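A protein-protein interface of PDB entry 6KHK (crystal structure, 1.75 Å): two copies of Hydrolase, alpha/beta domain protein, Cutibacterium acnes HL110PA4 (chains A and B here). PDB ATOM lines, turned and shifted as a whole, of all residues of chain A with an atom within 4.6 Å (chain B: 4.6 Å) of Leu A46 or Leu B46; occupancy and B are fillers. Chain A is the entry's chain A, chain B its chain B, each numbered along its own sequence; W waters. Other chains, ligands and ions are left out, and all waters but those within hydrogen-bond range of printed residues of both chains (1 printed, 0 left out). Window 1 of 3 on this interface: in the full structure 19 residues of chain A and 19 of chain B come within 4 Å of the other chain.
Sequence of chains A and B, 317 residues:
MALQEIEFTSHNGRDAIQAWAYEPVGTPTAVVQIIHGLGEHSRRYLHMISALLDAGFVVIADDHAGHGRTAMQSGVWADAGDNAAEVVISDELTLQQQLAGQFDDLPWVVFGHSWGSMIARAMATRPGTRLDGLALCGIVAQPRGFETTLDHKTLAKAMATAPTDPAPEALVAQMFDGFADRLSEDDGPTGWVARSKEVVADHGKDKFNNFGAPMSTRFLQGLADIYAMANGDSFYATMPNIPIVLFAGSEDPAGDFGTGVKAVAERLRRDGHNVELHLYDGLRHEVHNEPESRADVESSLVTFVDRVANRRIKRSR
Water W1 lies within hydrogen-bond range of NH1 of Arg B43 (3.0 Å) and NH1 of Arg A43 (3.0 Å).
Among the printed residues, merely in contact across the chains: Leu A46 with Leu B46 (3.5 Å), Leu A46 with Leu B53 (3.5 Å), His A47 with Ser B50 (3.8 Å), Ile A49 with Leu B46 (3.9 Å), Ser A50 with Leu B46 (3.9 Å), Ser A50 with His B47 (3.6 Å) and Leu A53 with Leu B46 (3.2 Å).
Printed residues of chain B within 4 Å of Leu A46: Leu B46 (3.5 Å) and Leu B53 (3.5 Å). Leu B46 touches just these residues of chain A: Leu A46 (3.5 Å), Ile A49 (3.9 Å), Ser A50 (3.9 Å) and Leu A53 (3.2 Å). Of the printed residues of chain B, Ser A50 touches Leu B46 and His B47. Of the printed residues of chain A, His B47 touches Ser A50 (3.6 Å). The nearest printed residue of chain B that does not touch Leu A46 is Ile B49 (4.01 Å).
Leu A46 touches Leu B53, and with the chains exchanged Leu A53 touches Leu B46. His A47 touches Ser B50, and with the chains exchanged Ser A50 touches His B47. Ile A49 touches Leu B46, but with the chains exchanged Leu A46 does not touch Ile B49 (4.01 Å). Ser A50 touches Leu B46, but with the chains exchanged Leu A46 does not touch Ser B50 (4.1 Å). Positions printed for both chains: 43, 44, 45, 46, 47, 48, 49, 50 and 53. Of the 7 pairs that touch across the chains among the printed residues, 5 have their exchanged pair printed and touching as well.
Of the 9 printed residues of chain A, 5 touch a printed residue of chain B. Along chain A the printed residues that touch a printed residue of chain B span positions 46 to 53. Printed residues of chain B that touch a printed residue of chain A: Leu B46, His B47, Ser B50 and Leu B53. Among the printed residues, 7 pairs touch across the chains. Among the printed residues, no Asp or Glu carboxylate lies within 4 Å of a Lys or Arg side-chain nitrogen of the other chain.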
ATOM      1  N   ARG A  43     -12.581   3.584  14.629  1.00  0.00           N
ATOM      2  CA  ARG A  43     -12.057   4.414  13.515  1.00  0.00           C
ATOM      3  C   ARG A  43     -13.180   5.346  13.013  1.00  0.00           C
ATOM      4  O   ARG A  43     -12.938   6.219  12.174  1.00  0.00           O
ATOM      5  CB  ARG A  43     -11.364   3.443  12.540  1.00  0.00           C
ATOM      6  CG  ARG A  43      -9.979   3.046  13.010  1.00  0.00           C
ATOM      7  CD  ARG A  43      -9.189   2.216  12.019  1.00  0.00           C
ATOM      8  NE  ARG A  43      -9.965   1.109  11.561  1.00  0.00           N
ATOM      9  CZ  ARG A  43      -9.641   0.304  10.568  1.00  0.00           C
ATOM     10  NH1 ARG A  43      -8.530   0.483   9.871  1.00  0.00           N
ATOM     11  NH2 ARG A  43     -10.445  -0.675  10.262  1.00  0.00           N
ATOM     12  N   ARG A  44     -14.359   5.173  13.566  1.00  0.00           N
ATOM     13  CA  ARG A  44     -15.530   6.034  13.301  1.00  0.00           C
ATOM     14  C   ARG A  44     -15.279   7.404  13.942  1.00  0.00           C
ATOM     15  O   ARG A  44     -15.942   8.331  13.609  1.00  0.00           O
ATOM     16  CB  ARG A  44     -16.726   5.356  13.980  1.00  0.00           C
ATOM     17  CG  ARG A  44     -18.064   5.726  13.394  1.00  0.00           C
ATOM     18  CD  ARG A  44     -19.238   4.847  13.744  1.00  0.00           C
ATOM     19  NE  ARG A  44     -20.352   5.667  13.341  1.00  0.00           N
ATOM     20  CZ  ARG A  44     -21.395   5.964  14.076  1.00  0.00           C
ATOM     21  NH1 ARG A  44     -21.525   5.454  15.277  1.00  0.00           N
ATOM     22  NH2 ARG A  44     -22.347   6.721  13.583  1.00  0.00           N
ATOM     23  N   TYR A  45     -14.313   7.452  14.849  1.00  0.00           N
ATOM     24  CA  TYR A  45     -14.041   8.659  15.653  1.00  0.00           C
ATOM     25  C   TYR A  45     -12.944   9.532  15.027  1.00  0.00           C
ATOM     26  O   TYR A  45     -12.335  10.221  15.740  1.00  0.00           O
ATOM     27  CB  TYR A  45     -13.594   8.228  17.047  1.00  0.00           C
ATOM     28  CG  TYR A  45     -14.742   7.717  17.871  1.00  0.00           C
ATOM     29  CD1 TYR A  45     -15.196   6.422  17.741  1.00  0.00           C
ATOM     30  CD2 TYR A  45     -15.390   8.548  18.761  1.00  0.00           C
ATOM     31  CE1 TYR A  45     -16.267   5.962  18.481  1.00  0.00           C
ATOM     32  CE2 TYR A  45     -16.467   8.105  19.508  1.00  0.00           C
ATOM     33  CZ  TYR A  45     -16.914   6.804  19.363  1.00  0.00           C
ATOM     34  OH  TYR A  45     -17.983   6.388  20.090  1.00  0.00           O
ATOM     35  N   LEU A  46     -12.724   9.423  13.730  1.00  0.00           N
ATOM     36  CA  LEU A  46     -11.649  10.197  13.063  1.00  0.00           C
ATOM     37  C   LEU A  46     -11.681  11.684  13.423  1.00  0.00           C
ATOM     38  O   LEU A  46     -10.657  12.210  13.747  1.00  0.00           O
ATOM     39  CB  LEU A  46     -11.835  10.092  11.557  1.00  0.00           C
ATOM     40  CG  LEU A  46     -10.600  10.496  10.784  1.00  0.00           C
ATOM     41  CD1 LEU A  46      -9.773   9.220  10.646  1.00  0.00           C
ATOM     42  CD2 LEU A  46     -10.982  10.955   9.398  1.00  0.00           C
ATOM     43  N   HIS A  47     -12.846  12.296  13.334  1.00  0.00           N
ATOM     44  CA  HIS A  47     -12.943  13.753  13.583  1.00  0.00           C
ATOM     45  C   HIS A  47     -12.474  14.068  15.011  1.00  0.00           C
ATOM     46  O   HIS A  47     -11.706  14.952  15.191  1.00  0.00           O
ATOM     47  CB  HIS A  47     -14.363  14.254  13.313  1.00  0.00           C
ATOM     48  CG  HIS A  47     -14.436  15.744  13.235  1.00  0.00           C
ATOM     49  ND1 HIS A  47     -14.506  16.539  14.345  1.00  0.00           N
ATOM     50  CD2 HIS A  47     -14.429  16.588  12.180  1.00  0.00           C
ATOM     51  CE1 HIS A  47     -14.546  17.789  13.986  1.00  0.00           C
ATOM     52  NE2 HIS A  47     -14.496  17.851  12.677  1.00  0.00           N
ATOM     53  N   MET A  48     -12.953  13.282  15.965  1.00  0.00           N
ATOM     54  CA  MET A  48     -12.589  13.496  17.386  1.00  0.00           C
ATOM     55  C   MET A  48     -11.085  13.256  17.564  1.00  0.00           C
ATOM     56  O   MET A  48     -10.420  14.013  18.288  1.00  0.00           O
ATOM     57  CB  MET A  48     -13.419  12.594  18.323  1.00  0.00           C
ATOM     58  CG  MET A  48     -13.136  12.860  19.748  1.00  0.00           C
ATOM     59  SD  MET A  48     -14.128  11.895  20.965  1.00  0.00           S
ATOM     60  CE  MET A  48     -15.463  13.071  21.022  1.00  0.00           C
ATOM     61  N   ILE A  49     -10.569  12.154  17.032  1.00  0.00           N
ATOM     62  CA  ILE A  49      -9.124  11.811  17.218  1.00  0.00           C
ATOM     63  C   ILE A  49      -8.290  12.991  16.715  1.00  0.00           C
ATOM     64  O   ILE A  49      -7.327  13.416  17.441  1.00  0.00           O
ATOM     65  CB  ILE A  49      -8.828  10.491  16.475  1.00  0.00           C
ATOM     66  CG1 ILE A  49      -9.582   9.350  17.151  1.00  0.00           C
ATOM     67  CG2 ILE A  49      -7.320  10.210  16.369  1.00  0.00           C
ATOM     68  CD1 ILE A  49      -9.637   8.095  16.361  1.00  0.00           C
ATOM     69  N   SER A  50      -8.574  13.423  15.503  1.00  0.00           N
ATOM     70  CA  SER A  50      -7.817  14.534  14.873  1.00  0.00           C
ATOM     71  C   SER A  50      -7.883  15.784  15.756  1.00  0.00           C
ATOM     72  O   SER A  50      -6.866  16.336  16.049  1.00  0.00           O
ATOM     73  CB  SER A  50      -8.302  14.825  13.479  1.00  0.00           C
ATOM     74  OG  SER A  50      -7.404  15.767  12.866  1.00  0.00           O
ATOM     75  N   LEU A  53      -5.704  15.267  18.782  1.00  0.00           N
ATOM     76  CA  LEU A  53      -4.274  15.406  18.366  1.00  0.00           C
ATOM     77  C   LEU A  53      -3.929  16.885  18.267  1.00  0.00           C
ATOM     78  O   LEU A  53      -2.785  17.257  18.754  1.00  0.00           O
ATOM     79  CB  LEU A  53      -4.018  14.666  17.046  1.00  0.00           C
ATOM     80  CG  LEU A  53      -4.102  13.144  17.147  1.00  0.00           C
ATOM     81  CD1 LEU A  53      -4.161  12.539  15.739  1.00  0.00           C
ATOM     82  CD2 LEU A  53      -2.967  12.569  17.948  1.00  0.00           C
ATOM     83  N   ARG B  43      -1.572   7.259   6.301  1.00  0.00           N
ATOM     84  CA  ARG B  43      -2.322   7.535   7.551  1.00  0.00           C
ATOM     85  C   ARG B  43      -1.646   8.681   8.340  1.00  0.00           C
ATOM     86  O   ARG B  43      -2.232   9.205   9.298  1.00  0.00           O
ATOM     87  CB  ARG B  43      -2.492   6.218   8.306  1.00  0.00           C
ATOM     88  CG  ARG B  43      -3.476   5.268   7.610  1.00  0.00           C
ATOM     89  CD  ARG B  43      -3.712   4.055   8.489  1.00  0.00           C
ATOM     90  NE  ARG B  43      -2.540   3.219   8.590  1.00  0.00           N
ATOM     91  CZ  ARG B  43      -2.485   2.070   9.281  1.00  0.00           C
ATOM     92  NH1 ARG B  43      -3.533   1.621   9.958  1.00  0.00           N
ATOM     93  NH2 ARG B  43      -1.350   1.400   9.348  1.00  0.00           N
ATOM     94  N   ARG B  44      -0.477   9.153   7.918  1.00  0.00           N
ATOM     95  CA  ARG B  44       0.158  10.401   8.398  1.00  0.00           C
ATOM     96  C   ARG B  44      -0.730  11.616   8.080  1.00  0.00           C
ATOM     97  O   ARG B  44      -0.587  12.612   8.762  1.00  0.00           O
ATOM     98  CB  ARG B  44       1.569  10.469   7.795  1.00  0.00           C
ATOM     99  CG  ARG B  44       2.393  11.563   8.386  1.00  0.00           C
ATOM    100  CD  ARG B  44       3.790  11.390   7.858  1.00  0.00           C
ATOM    101  NE  ARG B  44       4.612  12.282   8.605  1.00  0.00           N
ATOM    102  CZ  ARG B  44       5.330  13.262   8.039  1.00  0.00           C
ATOM    103  NH1 ARG B  44       5.477  13.307   6.728  1.00  0.00           N
ATOM    104  NH2 ARG B  44       6.035  14.070   8.804  1.00  0.00           N
ATOM    105  N   TYR B  45      -1.637  11.467   7.100  1.00  0.00           N
ATOM    106  CA  TYR B  45      -2.510  12.554   6.569  1.00  0.00           C
ATOM    107  C   TYR B  45      -3.860  12.671   7.301  1.00  0.00           C
ATOM    108  O   TYR B  45      -4.743  13.302   6.792  1.00  0.00           O
ATOM    109  CB  TYR B  45      -2.718  12.366   5.062  1.00  0.00           C
ATOM    110  CG  TYR B  45      -1.460  12.612   4.264  1.00  0.00           C
ATOM    111  CD1 TYR B  45      -0.425  11.703   4.239  1.00  0.00           C
ATOM    112  CD2 TYR B  45      -1.286  13.779   3.561  1.00  0.00           C
ATOM    113  CE1 TYR B  45       0.749  11.966   3.552  1.00  0.00           C
ATOM    114  CE2 TYR B  45      -0.126  14.051   2.860  1.00  0.00           C
ATOM    115  CZ  TYR B  45       0.901  13.139   2.848  1.00  0.00           C
ATOM    116  OH  TYR B  45       2.040  13.424   2.181  1.00  0.00           O
ATOM    117  N   LEU B  46      -3.965  12.114   8.501  1.00  0.00           N
ATOM    118  CA  LEU B  46      -5.219  12.152   9.299  1.00  0.00           C
ATOM    119  C   LEU B  46      -5.826  13.567   9.364  1.00  0.00           C
ATOM    120  O   LEU B  46      -7.003  13.695   9.111  1.00  0.00           O
ATOM    121  CB  LEU B  46      -4.886  11.645  10.707  1.00  0.00           C
ATOM    122  CG  LEU B  46      -6.033  11.332  11.646  1.00  0.00           C
ATOM    123  CD1 LEU B  46      -5.699  11.654  13.089  1.00  0.00           C
ATOM    124  CD2 LEU B  46      -7.364  11.848  11.190  1.00  0.00           C
ATOM    125  N   HIS B  47      -5.017  14.578   9.641  1.00  0.00           N
ATOM    126  CA  HIS B  47      -5.574  15.954   9.738  1.00  0.00           C
ATOM    127  C   HIS B  47      -6.225  16.370   8.412  1.00  0.00           C
ATOM    128  O   HIS B  47      -7.360  16.797   8.440  1.00  0.00           O
ATOM    129  CB  HIS B  47      -4.535  16.987  10.166  1.00  0.00           C
ATOM    130  CG  HIS B  47      -5.128  18.315  10.523  1.00  0.00           C
ATOM    131  ND1 HIS B  47      -5.415  19.271   9.598  1.00  0.00           N
ATOM    132  CD2 HIS B  47      -5.489  18.849  11.707  1.00  0.00           C
ATOM    133  CE1 HIS B  47      -5.914  20.329  10.189  1.00  0.00           C
ATOM    134  NE2 HIS B  47      -5.961  20.099  11.471  1.00  0.00           N
ATOM    135  N   MET B  48      -5.474  16.273   7.325  1.00  0.00           N
ATOM    136  CA  MET B  48      -5.927  16.605   5.941  1.00  0.00           C
ATOM    137  C   MET B  48      -7.137  15.744   5.621  1.00  0.00           C
ATOM    138  O   MET B  48      -8.094  16.311   5.110  1.00  0.00           O
ATOM    139  CB  MET B  48      -4.853  16.449   4.840  1.00  0.00           C
ATOM    140  CG  MET B  48      -5.374  16.604   3.403  1.00  0.00           C
ATOM    141  SD  MET B  48      -4.014  16.710   2.164  1.00  0.00           S
ATOM    142  CE  MET B  48      -3.506  18.405   2.379  1.00  0.00           C
ATOM    143  N   ILE B  49      -7.108  14.405   5.835  1.00  0.00           N
ATOM    144  CA  ILE B  49      -8.270  13.544   5.494  1.00  0.00           C
ATOM    145  C   ILE B  49      -9.525  14.109   6.185  1.00  0.00           C
ATOM    146  O   ILE B  49     -10.607  14.127   5.583  1.00  0.00           O
ATOM    147  CB  ILE B  49      -7.998  12.073   5.874  1.00  0.00           C
ATOM    148  CG1 ILE B  49      -6.848  11.521   5.021  1.00  0.00           C
ATOM    149  CG2 ILE B  49      -9.272  11.251   5.781  1.00  0.00           C
ATOM    150  CD1 ILE B  49      -6.150  10.298   5.545  1.00  0.00           C
ATOM    151  N   SER B  50      -9.407  14.470   7.449  1.00  0.00           N
ATOM    152  CA  SER B  50     -10.550  14.916   8.279  1.00  0.00           C
ATOM    153  C   SER B  50     -11.076  16.257   7.743  1.00  0.00           C
ATOM    154  O   SER B  50     -12.288  16.393   7.673  1.00  0.00           O
ATOM    155  CB  SER B  50     -10.133  15.030   9.721  1.00  0.00           C
ATOM    156  OG  SER B  50     -11.273  15.295  10.526  1.00  0.00           O
ATOM    157  N   LEU B  53     -12.984  15.374   4.466  1.00  0.00           N
ATOM    158  CA  LEU B  53     -14.293  14.794   4.846  1.00  0.00           C
ATOM    159  C   LEU B  53     -15.223  15.921   5.301  1.00  0.00           C
ATOM    160  O   LEU B  53     -16.420  15.875   4.960  1.00  0.00           O
ATOM    161  CB  LEU B  53     -14.134  13.737   5.941  1.00  0.00           C
ATOM    162  CG  LEU B  53     -13.442  12.435   5.509  1.00  0.00           C
ATOM    163  CD1 LEU B  53     -13.109  11.600   6.726  1.00  0.00           C
ATOM    164  CD2 LEU B  53     -14.243  11.609   4.538  1.00  0.00           C
HETATM  165  O   HOH W   1      -6.384   2.602  10.115  1.00  0.00           O
